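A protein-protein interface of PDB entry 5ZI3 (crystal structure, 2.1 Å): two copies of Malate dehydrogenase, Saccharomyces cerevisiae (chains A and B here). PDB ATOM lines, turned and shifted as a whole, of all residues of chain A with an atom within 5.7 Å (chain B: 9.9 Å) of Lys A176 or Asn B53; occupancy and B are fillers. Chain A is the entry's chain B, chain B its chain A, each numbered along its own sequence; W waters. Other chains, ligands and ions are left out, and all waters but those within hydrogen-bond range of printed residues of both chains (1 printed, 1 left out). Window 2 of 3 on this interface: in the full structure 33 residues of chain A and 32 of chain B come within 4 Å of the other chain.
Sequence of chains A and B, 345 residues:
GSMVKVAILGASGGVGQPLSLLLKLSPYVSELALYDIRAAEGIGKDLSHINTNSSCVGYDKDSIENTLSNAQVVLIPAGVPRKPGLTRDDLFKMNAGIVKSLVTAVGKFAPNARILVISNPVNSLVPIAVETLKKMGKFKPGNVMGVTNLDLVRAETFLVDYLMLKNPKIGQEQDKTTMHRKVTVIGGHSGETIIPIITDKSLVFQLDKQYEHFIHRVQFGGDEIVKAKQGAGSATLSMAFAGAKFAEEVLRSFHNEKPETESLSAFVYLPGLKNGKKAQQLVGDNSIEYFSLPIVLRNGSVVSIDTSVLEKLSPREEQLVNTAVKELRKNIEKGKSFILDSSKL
No position is printed for both chains.
The backbone carbonyl oxygen (O) of Lys B24 sits at hydrogen-bond distance from the side-chain hydroxyl (OG1) of Thr B52 (2.7 Å). OD1 of Asp A175 lies within hydrogen-bond range of OG1 of Thr A177, at 2.5 Å. The side-chain carboxylate (OE1) of Glu A156 lies within hydrogen-bond range of the backbone NH (N) of His A180 (3.0 Å). The side-chain carboxylate (OE1) of Glu A156 is in hydrogen-bond range of the backbone NH (N) of Met A179, at 3.5 Å. NZ of Lys A176 is in salt-bridge range of OD1 of Asp A161.
Water W1 bridges OD2 of Asp A161 (2.5 Å) and O of Ser B48 (3.1 Å).
Thr A157 touches Ser B48. CD of Lys A176 touches O of Thr B52, 3.5 Å away.
Of the 11 printed residues of chain A, 5 touch a printed residue of chain B. Among the printed residues, 10 pairs touch across the chains. Among the printed residues, no Asp or Glu carboxylate lies within 4 Å of a Lys or Arg side-chain nitrogen of the other chain.
The side-chain amide nitrogen of Asn B53 is in hydrogen-bond range of the side-chain carboxylate of Asp A175 (2.9 Å). The side-chain hydroxyl of Thr A157 sits close to the backbone NH of Asn B51, 3.2 Å away. OG1 of Thr A157 sits at hydrogen-bond distance from O of His B49 (2.7 Å). ND2 of Asn B51 sits at hydrogen-bond distance from O of Lys A176, 3.2 Å away. The backbone carbonyl oxygen (O) of Asn B51 is in hydrogen-bond range of the backbone NH (N) of Thr A177 (3.3 Å). The side-chain amide oxygen (OD1) of Asn B53 is in hydrogen-bond range of the backbone NH (N) of Lys A176 (2.9 Å). OE1 of Glu A156 is in hydrogen-bond range of ND2 of Asn B51, at 3.3 Å. O of Ile B50 sits close to OG1 of Thr A157 (3.4 Å).
Of the printed residues of chain B, Lys A176 touches Asn B51, Thr B52 and Asn B53. Asn B53 touches just these residues of chain A: Asp A175 and Lys A176. Printed residues of chain B within 4 Å of Asp A175: Asn B53 (2.9 Å). Of chain B, only Asn B51 (3.3 Å) comes within 4 Å of Thr A177. Printed residues of chain A within 4 Å of His B49: Thr A157 (2.7 Å). Of the printed residues of chain A, Ser B48 touches Thr A157 (3.5 Å). Printed residues of chain A within 4 Å of Ile B50: Thr A157 (3.3 Å). Of the printed residues of chain A, Asn B51 touches Glu A156 (3.3 Å), Thr A157 (3.1 Å), Lys A176 (3.2 Å) and Thr A177 (3.3 Å). Of the printed residues of chain A, Thr B52 touches Lys A176 (3.5 Å). The nearest residue of chain B that does not touch Lys A176 is Ile B50 (4.8 Å). The nearest residue of chain A that does not touch Asn B53 is Gln A174 (4.2 Å). The nearest printed residue of chain A that does not touch His B49 is Glu A156 (6.5 Å).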
ATOM      1  N   GLU A 156      -5.234 -29.984  22.288  1.00  0.00           N
ATOM      2  CA  GLU A 156      -4.187 -30.015  21.279  1.00  0.00           C
ATOM      3  C   GLU A 156      -3.854 -28.620  20.784  1.00  0.00           C
ATOM      4  O   GLU A 156      -2.686 -28.260  20.677  1.00  0.00           O
ATOM      5  CB  GLU A 156      -4.609 -30.887  20.126  1.00  0.00           C
ATOM      6  CG  GLU A 156      -4.697 -32.353  20.509  1.00  0.00           C
ATOM      7  CD  GLU A 156      -5.148 -33.256  19.376  1.00  0.00           C
ATOM      8  OE1 GLU A 156      -4.320 -33.561  18.509  1.00  0.00           O
ATOM      9  OE2 GLU A 156      -6.307 -33.700  19.379  1.00  0.00           O
ATOM     10  N   THR A 157      -4.900 -27.810  20.555  1.00  0.00           N
ATOM     11  CA  THR A 157      -4.730 -26.473  20.005  1.00  0.00           C
ATOM     12  C   THR A 157      -4.067 -25.593  21.031  1.00  0.00           C
ATOM     13  O   THR A 157      -3.102 -24.920  20.711  1.00  0.00           O
ATOM     14  CB  THR A 157      -6.064 -25.839  19.592  1.00  0.00           C
ATOM     15  OG1 THR A 157      -6.616 -26.631  18.536  1.00  0.00           O
ATOM     16  CG2 THR A 157      -5.829 -24.416  19.096  1.00  0.00           C
ATOM     17  N   VAL A 160      -0.188 -26.055  22.056  1.00  0.00           N
ATOM     18  CA  VAL A 160       0.661 -25.363  21.122  1.00  0.00           C
ATOM     19  C   VAL A 160       0.593 -23.865  21.343  1.00  0.00           C
ATOM     20  O   VAL A 160       1.637 -23.216  21.415  1.00  0.00           O
ATOM     21  CB  VAL A 160       0.303 -25.652  19.657  1.00  0.00           C
ATOM     22  CG1 VAL A 160       1.063 -24.732  18.717  1.00  0.00           C
ATOM     23  CG2 VAL A 160       0.542 -27.119  19.318  1.00  0.00           C
ATOM     24  N   ASP A 161      -0.605 -23.311  21.507  1.00  0.00           N
ATOM     25  CA  ASP A 161      -0.719 -21.869  21.669  1.00  0.00           C
ATOM     26  C   ASP A 161       0.019 -21.430  22.944  1.00  0.00           C
ATOM     27  O   ASP A 161       0.674 -20.395  22.948  1.00  0.00           O
ATOM     28  CB  ASP A 161      -2.173 -21.359  21.802  1.00  0.00           C
ATOM     29  CG  ASP A 161      -3.038 -21.561  20.548  1.00  0.00           C
ATOM     30  OD1 ASP A 161      -2.577 -21.619  19.401  1.00  0.00           O
ATOM     31  OD2 ASP A 161      -4.242 -21.679  20.743  1.00  0.00           O
ATOM     32  N   GLN A 174       5.842 -27.697  17.268  1.00  0.00           N
ATOM     33  CA  GLN A 174       4.642 -28.510  17.423  1.00  0.00           C
ATOM     34  C   GLN A 174       3.785 -28.455  16.180  1.00  0.00           C
ATOM     35  O   GLN A 174       3.724 -27.487  15.447  1.00  0.00           O
ATOM     36  CB  GLN A 174       3.811 -28.065  18.617  1.00  0.00           C
ATOM     37  CG  GLN A 174       4.625 -27.872  19.890  1.00  0.00           C
ATOM     38  CD  GLN A 174       5.390 -29.117  20.268  1.00  0.00           C
ATOM     39  OE1 GLN A 174       4.804 -30.202  20.381  1.00  0.00           O
ATOM     40  NE2 GLN A 174       6.701 -28.984  20.457  1.00  0.00           N
ATOM     41  N   ASP A 175       3.087 -29.529  15.963  1.00  0.00           N
ATOM     42  CA  ASP A 175       2.158 -29.586  14.933  1.00  0.00           C
ATOM     43  C   ASP A 175       0.794 -29.761  15.615  1.00  0.00           C
ATOM     44  O   ASP A 175       0.547 -30.767  16.225  1.00  0.00           O
ATOM     45  CB  ASP A 175       2.518 -30.781  14.054  1.00  0.00           C
ATOM     46  CG  ASP A 175       1.540 -30.966  12.968  1.00  0.00           C
ATOM     47  OD1 ASP A 175       0.485 -30.281  13.030  1.00  0.00           O
ATOM     48  OD2 ASP A 175       1.810 -31.779  12.076  1.00  0.00           O
ATOM     49  N   LYS A 176      -0.112 -28.803  15.465  1.00  0.00           N
ATOM     50  CA  LYS A 176      -1.393 -28.958  16.156  1.00  0.00           C
ATOM     51  C   LYS A 176      -2.133 -30.240  15.779  1.00  0.00           C
ATOM     52  O   LYS A 176      -2.801 -30.824  16.605  1.00  0.00           O
ATOM     53  CB  LYS A 176      -2.268 -27.736  15.933  1.00  0.00           C
ATOM     54  CG  LYS A 176      -1.841 -26.510  16.733  1.00  0.00           C
ATOM     55  CD  LYS A 176      -2.723 -25.316  16.398  1.00  0.00           C
ATOM     56  CE  LYS A 176      -2.263 -24.124  17.218  1.00  0.00           C
ATOM     57  NZ  LYS A 176      -3.111 -22.954  16.985  1.00  0.00           N
ATOM     58  N   THR A 177      -2.009 -30.680  14.522  1.00  0.00           N
ATOM     59  CA  THR A 177      -2.675 -31.899  14.024  1.00  0.00           C
ATOM     60  C   THR A 177      -2.193 -33.185  14.710  1.00  0.00           C
ATOM     61  O   THR A 177      -2.932 -34.166  14.713  1.00  0.00           O
ATOM     62  CB  THR A 177      -2.472 -32.103  12.496  1.00  0.00           C
ATOM     63  OG1 THR A 177      -1.062 -32.106  12.227  1.00  0.00           O
ATOM     64  CG2 THR A 177      -3.131 -30.958  11.698  1.00  0.00           C
ATOM     65  N   THR A 178      -0.984 -33.197  15.280  1.00  0.00           N
ATOM     66  CA  THR A 178      -0.459 -34.436  15.894  1.00  0.00           C
ATOM     67  C   THR A 178      -0.256 -34.399  17.445  1.00  0.00           C
ATOM     68  O   THR A 178       0.395 -35.267  18.002  1.00  0.00           O
ATOM     69  CB  THR A 178       0.857 -34.887  15.212  1.00  0.00           C
ATOM     70  OG1 THR A 178       1.880 -33.949  15.505  1.00  0.00           O
ATOM     71  CG2 THR A 178       0.731 -34.980  13.661  1.00  0.00           C
ATOM     72  N   MET A 179      -0.865 -33.440  18.133  1.00  0.00           N
ATOM     73  CA  MET A 179      -0.634 -33.216  19.544  1.00  0.00           C
ATOM     74  C   MET A 179      -1.284 -34.225  20.508  1.00  0.00           C
ATOM     75  O   MET A 179      -0.944 -34.253  21.712  1.00  0.00           O
ATOM     76  CB  MET A 179      -1.095 -31.805  19.905  1.00  0.00           C
ATOM     77  CG  MET A 179      -0.275 -30.701  19.356  1.00  0.00           C
ATOM     78  SD  MET A 179       1.458 -30.872  19.926  1.00  0.00           S
ATOM     79  CE  MET A 179       1.345 -30.511  21.649  1.00  0.00           C
ATOM     80  N   HIS A 180      -2.222 -35.016  20.007  1.00  0.00           N
ATOM     81  CA  HIS A 180      -2.811 -36.104  20.764  1.00  0.00           C
ATOM     82  C   HIS A 180      -1.834 -37.194  21.230  1.00  0.00           C
ATOM     83  O   HIS A 180      -2.177 -37.984  22.114  1.00  0.00           O
ATOM     84  CB  HIS A 180      -3.901 -36.786  19.944  1.00  0.00           C
ATOM     85  CG  HIS A 180      -3.438 -37.258  18.611  1.00  0.00           C
ATOM     86  ND1 HIS A 180      -2.798 -38.469  18.434  1.00  0.00           N
ATOM     87  CD2 HIS A 180      -3.502 -36.680  17.392  1.00  0.00           C
ATOM     88  CE1 HIS A 180      -2.490 -38.616  17.159  1.00  0.00           C
ATOM     89  NE2 HIS A 180      -2.908 -37.545  16.504  1.00  0.00           N
ATOM     90  N   MET B   3       1.751 -21.187   4.362  1.00  0.00           N
ATOM     91  CA  MET B   3       2.629 -20.046   3.960  1.00  0.00           C
ATOM     92  C   MET B   3       1.893 -18.727   3.632  1.00  0.00           C
ATOM     93  O   MET B   3       2.445 -17.665   3.851  1.00  0.00           O
ATOM     94  CB  MET B   3       3.473 -20.459   2.758  1.00  0.00           C
ATOM     95  CG  MET B   3       4.700 -19.601   2.572  1.00  0.00           C
ATOM     96  SD  MET B   3       5.959 -20.467   1.615  1.00  0.00           S
ATOM     97  CE  MET B   3       6.353 -21.859   2.684  1.00  0.00           C
ATOM     98  N   VAL B   4       0.656 -18.811   3.134  1.00  0.00           N
ATOM     99  CA  VAL B   4      -0.107 -17.677   2.566  1.00  0.00           C
ATOM    100  C   VAL B   4      -1.307 -17.210   3.427  1.00  0.00           C
ATOM    101  O   VAL B   4      -2.018 -18.049   3.940  1.00  0.00           O
ATOM    102  CB  VAL B   4      -0.685 -18.159   1.237  1.00  0.00           C
ATOM    103  CG1 VAL B   4      -1.955 -17.404   0.879  1.00  0.00           C
ATOM    104  CG2 VAL B   4       0.354 -18.048   0.139  1.00  0.00           C
ATOM    105  N   LEU B  23     -11.848 -23.947   4.927  1.00  0.00           N
ATOM    106  CA  LEU B  23     -10.607 -23.225   4.849  1.00  0.00           C
ATOM    107  C   LEU B  23      -9.743 -23.361   6.121  1.00  0.00           C
ATOM    108  O   LEU B  23      -8.566 -23.479   5.981  1.00  0.00           O
ATOM    109  CB  LEU B  23     -10.796 -21.764   4.458  1.00  0.00           C
ATOM    110  CG  LEU B  23     -10.574 -21.434   2.951  1.00  0.00           C
ATOM    111  CD1 LEU B  23      -9.118 -21.431   2.589  1.00  0.00           C
ATOM    112  CD2 LEU B  23     -11.248 -22.412   2.063  1.00  0.00           C
ATOM    113  N   LYS B  24     -10.320 -23.379   7.326  1.00  0.00           N
ATOM    114  CA  LYS B  24      -9.519 -23.674   8.528  1.00  0.00           C
ATOM    115  C   LYS B  24      -8.783 -25.016   8.466  1.00  0.00           C
ATOM    116  O   LYS B  24      -7.691 -25.138   9.014  1.00  0.00           O
ATOM    117  CB  LYS B  24     -10.366 -23.668   9.788  1.00  0.00           C
ATOM    118  CG  LYS B  24      -9.582 -23.914  11.085  1.00  0.00           C
ATOM    119  CD  LYS B  24      -8.648 -22.755  11.363  1.00  0.00           C
ATOM    120  CE  LYS B  24      -7.985 -22.902  12.728  1.00  0.00           C
ATOM    121  NZ  LYS B  24      -6.643 -23.500  12.647  1.00  0.00           N
ATOM    122  N   LEU B  25      -9.379 -26.011   7.828  1.00  0.00           N
ATOM    123  CA  LEU B  25      -8.747 -27.288   7.689  1.00  0.00           C
ATOM    124  C   LEU B  25      -7.576 -27.363   6.692  1.00  0.00           C
ATOM    125  O   LEU B  25      -6.902 -28.382   6.625  1.00  0.00           O
ATOM    126  CB  LEU B  25      -9.774 -28.319   7.287  1.00  0.00           C
ATOM    127  CG  LEU B  25     -10.981 -28.377   8.195  1.00  0.00           C
ATOM    128  CD1 LEU B  25     -11.771 -29.586   7.845  1.00  0.00           C
ATOM    129  CD2 LEU B  25     -10.522 -28.417   9.638  1.00  0.00           C
ATOM    130  N   SER B  26      -7.361 -26.344   5.864  1.00  0.00           N
ATOM    131  CA  SER B  26      -6.371 -26.481   4.795  1.00  0.00           C
ATOM    132  C   SER B  26      -4.935 -26.392   5.316  1.00  0.00           C
ATOM    133  O   SER B  26      -4.575 -25.421   5.946  1.00  0.00           O
ATOM    134  CB  SER B  26      -6.552 -25.409   3.705  1.00  0.00           C
ATOM    135  OG  SER B  26      -5.380 -25.323   2.876  1.00  0.00           O
ATOM    136  N   PRO B  27      -4.070 -27.353   4.947  1.00  0.00           N
ATOM    137  CA  PRO B  27      -2.679 -27.178   5.361  1.00  0.00           C
ATOM    138  C   PRO B  27      -1.917 -26.103   4.589  1.00  0.00           C
ATOM    139  O   PRO B  27      -0.795 -25.829   4.941  1.00  0.00           O
ATOM    140  CB  PRO B  27      -2.058 -28.568   5.121  1.00  0.00           C
ATOM    141  CG  PRO B  27      -2.895 -29.153   4.028  1.00  0.00           C
ATOM    142  CD  PRO B  27      -4.308 -28.667   4.318  1.00  0.00           C
ATOM    143  N   TYR B  28      -2.503 -25.469   3.575  1.00  0.00           N
ATOM    144  CA  TYR B  28      -1.787 -24.463   2.785  1.00  0.00           C
ATOM    145  C   TYR B  28      -1.986 -23.061   3.275  1.00  0.00           C
ATOM    146  O   TYR B  28      -1.498 -22.118   2.679  1.00  0.00           O
ATOM    147  CB  TYR B  28      -2.239 -24.522   1.311  1.00  0.00           C
ATOM    148  CG  TYR B  28      -1.937 -25.832   0.627  1.00  0.00           C
ATOM    149  CD1 TYR B  28      -0.701 -26.063   0.033  1.00  0.00           C
ATOM    150  CD2 TYR B  28      -2.869 -26.824   0.573  1.00  0.00           C
ATOM    151  CE1 TYR B  28      -0.412 -27.288  -0.580  1.00  0.00           C
ATOM    152  CE2 TYR B  28      -2.603 -28.033  -0.039  1.00  0.00           C
ATOM    153  CZ  TYR B  28      -1.379 -28.261  -0.615  1.00  0.00           C
ATOM    154  OH  TYR B  28      -1.144 -29.464  -1.213  1.00  0.00           O
ATOM    155  N   VAL B  29      -2.699 -22.909   4.371  1.00  0.00           N
ATOM    156  CA  VAL B  29      -3.034 -21.591   4.873  1.00  0.00           C
ATOM    157  C   VAL B  29      -2.258 -21.319   6.129  1.00  0.00           C
ATOM    158  O   VAL B  29      -2.275 -22.135   7.023  1.00  0.00           O
ATOM    159  CB  VAL B  29      -4.543 -21.531   5.236  1.00  0.00           C
ATOM    160  CG1 VAL B  29      -4.911 -20.151   5.786  1.00  0.00           C
ATOM    161  CG2 VAL B  29      -5.390 -21.866   4.033  1.00  0.00           C
ATOM    162  N   SER B  30      -1.646 -20.145   6.218  1.00  0.00           N
ATOM    163  CA  SER B  30      -0.898 -19.749   7.387  1.00  0.00           C
ATOM    164  C   SER B  30      -1.776 -18.902   8.302  1.00  0.00           C
ATOM    165  O   SER B  30      -1.728 -19.032   9.516  1.00  0.00           O
ATOM    166  CB  SER B  30       0.315 -18.907   6.968  1.00  0.00           C
ATOM    167  OG  SER B  30      -0.092 -17.692   6.321  1.00  0.00           O
ATOM    168  N   GLU B  31      -2.532 -17.991   7.684  1.00  0.00           N
ATOM    169  CA  GLU B  31      -3.382 -17.052   8.382  1.00  0.00           C
ATOM    170  C   GLU B  31      -4.711 -17.001   7.692  1.00  0.00           C
ATOM    171  O   GLU B  31      -4.780 -16.923   6.479  1.00  0.00           O
ATOM    172  CB  GLU B  31      -2.759 -15.653   8.354  1.00  0.00           C
ATOM    173  CG  GLU B  31      -1.704 -15.398   9.403  1.00  0.00           C
ATOM    174  CD  GLU B  31      -1.177 -13.983   9.294  1.00  0.00           C
ATOM    175  OE1 GLU B  31      -0.684 -13.642   8.206  1.00  0.00           O
ATOM    176  OE2 GLU B  31      -1.286 -13.213  10.270  1.00  0.00           O
ATOM    177  N   LEU B  32      -5.775 -17.103   8.474  1.00  0.00           N
ATOM    178  CA  LEU B  32      -7.089 -17.070   7.941  1.00  0.00           C
ATOM    179  C   LEU B  32      -7.846 -15.913   8.617  1.00  0.00           C
ATOM    180  O   LEU B  32      -8.098 -15.961   9.818  1.00  0.00           O
ATOM    181  CB  LEU B  32      -7.786 -18.420   8.191  1.00  0.00           C
ATOM    182  CG  LEU B  32      -9.252 -18.481   7.728  1.00  0.00           C
ATOM    183  CD1 LEU B  32      -9.338 -18.177   6.259  1.00  0.00           C
ATOM    184  CD2 LEU B  32      -9.971 -19.782   8.036  1.00  0.00           C
ATOM    185  N   LEU B  47     -13.586 -21.203  15.237  1.00  0.00           N
ATOM    186  CA  LEU B  47     -12.697 -21.902  14.348  1.00  0.00           C
ATOM    187  C   LEU B  47     -11.259 -21.900  14.862  1.00  0.00           C
ATOM    188  O   LEU B  47     -10.555 -22.853  14.625  1.00  0.00           O
ATOM    189  CB  LEU B  47     -12.741 -21.307  12.956  1.00  0.00           C
ATOM    190  CG  LEU B  47     -13.999 -21.537  12.148  1.00  0.00           C
ATOM    191  CD1 LEU B  47     -13.955 -20.734  10.866  1.00  0.00           C
ATOM    192  CD2 LEU B  47     -14.266 -23.011  11.856  1.00  0.00           C
ATOM    193  N   SER B  48     -10.833 -20.876  15.583  1.00  0.00           N
ATOM    194  CA  SER B  48      -9.455 -20.846  16.164  1.00  0.00           C
ATOM    195  C   SER B  48      -9.163 -22.017  17.147  1.00  0.00           C
ATOM    196  O   SER B  48      -7.986 -22.362  17.348  1.00  0.00           O
ATOM    197  CB  SER B  48      -9.152 -19.517  16.872  1.00  0.00           C
ATOM    198  OG  SER B  48      -9.908 -19.445  18.101  1.00  0.00           O
ATOM    199  N   HIS B  49     -10.197 -22.655  17.702  1.00  0.00           N
ATOM    200  CA  HIS B  49     -10.016 -23.843  18.523  1.00  0.00           C
ATOM    201  C   HIS B  49      -9.705 -25.142  17.798  1.00  0.00           C
ATOM    202  O   HIS B  49      -9.308 -26.081  18.454  1.00  0.00           O
ATOM    203  CB  HIS B  49     -11.191 -24.112  19.460  1.00  0.00           C
ATOM    204  CG  HIS B  49     -11.406 -23.019  20.413  1.00  0.00           C
ATOM    205  ND1 HIS B  49     -12.317 -23.100  21.437  1.00  0.00           N
ATOM    206  CD2 HIS B  49     -10.777 -21.826  20.546  1.00  0.00           C
ATOM    207  CE1 HIS B  49     -12.260 -21.988  22.149  1.00  0.00           C
ATOM    208  NE2 HIS B  49     -11.328 -21.207  21.631  1.00  0.00           N
ATOM    209  N   ILE B  50      -9.823 -25.164  16.469  1.00  0.00           N
ATOM    210  CA  ILE B  50      -9.617 -26.372  15.693  1.00  0.00           C
ATOM    211  C   ILE B  50      -8.119 -26.588  15.603  1.00  0.00           C
ATOM    212  O   ILE B  50      -7.351 -25.671  15.335  1.00  0.00           O
ATOM    213  CB  ILE B  50     -10.244 -26.263  14.283  1.00  0.00           C
ATOM    214  CG1 ILE B  50     -11.764 -26.382  14.404  1.00  0.00           C
ATOM    215  CG2 ILE B  50      -9.718 -27.336  13.318  1.00  0.00           C
ATOM    216  CD1 ILE B  50     -12.526 -26.155  13.118  1.00  0.00           C
ATOM    217  N   ASN B  51      -7.703 -27.814  15.778  1.00  0.00           N
ATOM    218  CA  ASN B  51      -6.254 -28.098  15.865  1.00  0.00           C
ATOM    219  C   ASN B  51      -5.610 -28.328  14.494  1.00  0.00           C
ATOM    220  O   ASN B  51      -5.088 -29.435  14.225  1.00  0.00           O
ATOM    221  CB  ASN B  51      -6.033 -29.282  16.797  1.00  0.00           C
ATOM    222  CG  ASN B  51      -6.657 -30.568  16.278  1.00  0.00           C
ATOM    223  OD1 ASN B  51      -7.828 -30.597  15.914  1.00  0.00           O
ATOM    224  ND2 ASN B  51      -5.870 -31.646  16.260  1.00  0.00           N
ATOM    225  N   THR B  52      -5.659 -27.277  13.644  1.00  0.00           N
ATOM    226  CA  THR B  52      -4.955 -27.217  12.359  1.00  0.00           C
ATOM    227  C   THR B  52      -4.076 -25.976  12.512  1.00  0.00           C
ATOM    228  O   THR B  52      -4.360 -25.093  13.367  1.00  0.00           O
ATOM    229  CB  THR B  52      -5.926 -27.065  11.151  1.00  0.00           C
ATOM    230  OG1 THR B  52      -6.792 -25.958  11.420  1.00  0.00           O
ATOM    231  CG2 THR B  52      -6.740 -28.296  10.964  1.00  0.00           C
ATOM    232  N   ASN B  53      -2.998 -25.885  11.727  1.00  0.00           N
ATOM    233  CA  ASN B  53      -1.934 -24.917  12.018  1.00  0.00           C
ATOM    234  C   ASN B  53      -2.178 -23.443  11.679  1.00  0.00           C
ATOM    235  O   ASN B  53      -1.520 -22.562  12.233  1.00  0.00           O
ATOM    236  CB  ASN B  53      -0.591 -25.450  11.495  1.00  0.00           C
ATOM    237  CG  ASN B  53      -0.139 -26.657  12.320  1.00  0.00           C
ATOM    238  OD1 ASN B  53       0.047 -26.564  13.571  1.00  0.00           O
ATOM    239  ND2 ASN B  53      -0.088 -27.813  11.673  1.00  0.00           N
ATOM    240  N   SER B  54      -3.185 -23.161  10.884  1.00  0.00           N
ATOM    241  CA  SER B  54      -3.541 -21.763  10.565  1.00  0.00           C
ATOM    242  C   SER B  54      -4.005 -20.966  11.782  1.00  0.00           C
ATOM    243  O   SER B  54      -4.675 -21.490  12.662  1.00  0.00           O
ATOM    244  CB  SER B  54      -4.636 -21.739   9.530  1.00  0.00           C
ATOM    245  OG  SER B  54      -5.688 -22.545   9.979  1.00  0.00           O
ATOM    246  N   SER B  55      -3.640 -19.695  11.789  1.00  0.00           N
ATOM    247  CA  SER B  55      -4.061 -18.747  12.779  1.00  0.00           C
ATOM    248  C   SER B  55      -5.350 -18.082  12.241  1.00  0.00           C
ATOM    249  O   SER B  55      -5.320 -17.409  11.196  1.00  0.00           O
ATOM    250  CB  SER B  55      -2.916 -17.737  12.954  1.00  0.00           C
ATOM    251  OG  SER B  55      -3.342 -16.537  13.503  1.00  0.00           O
ATOM    252  N   CYS B  56      -6.461 -18.250  12.953  1.00  0.00           N
ATOM    253  CA  CYS B  56      -7.789 -17.806  12.476  1.00  0.00           C
ATOM    254  C   CYS B  56      -8.304 -16.699  13.347  1.00  0.00           C
ATOM    255  O   CYS B  56      -8.499 -16.906  14.565  1.00  0.00           O
ATOM    256  CB  CYS B  56      -8.829 -18.953  12.489  1.00  0.00           C
ATOM    257  SG  CYS B  56     -10.426 -18.503  11.725  1.00  0.00           S
HETATM  258  O   HOH W   1      -5.896 -20.936  19.056  1.00  0.00           O
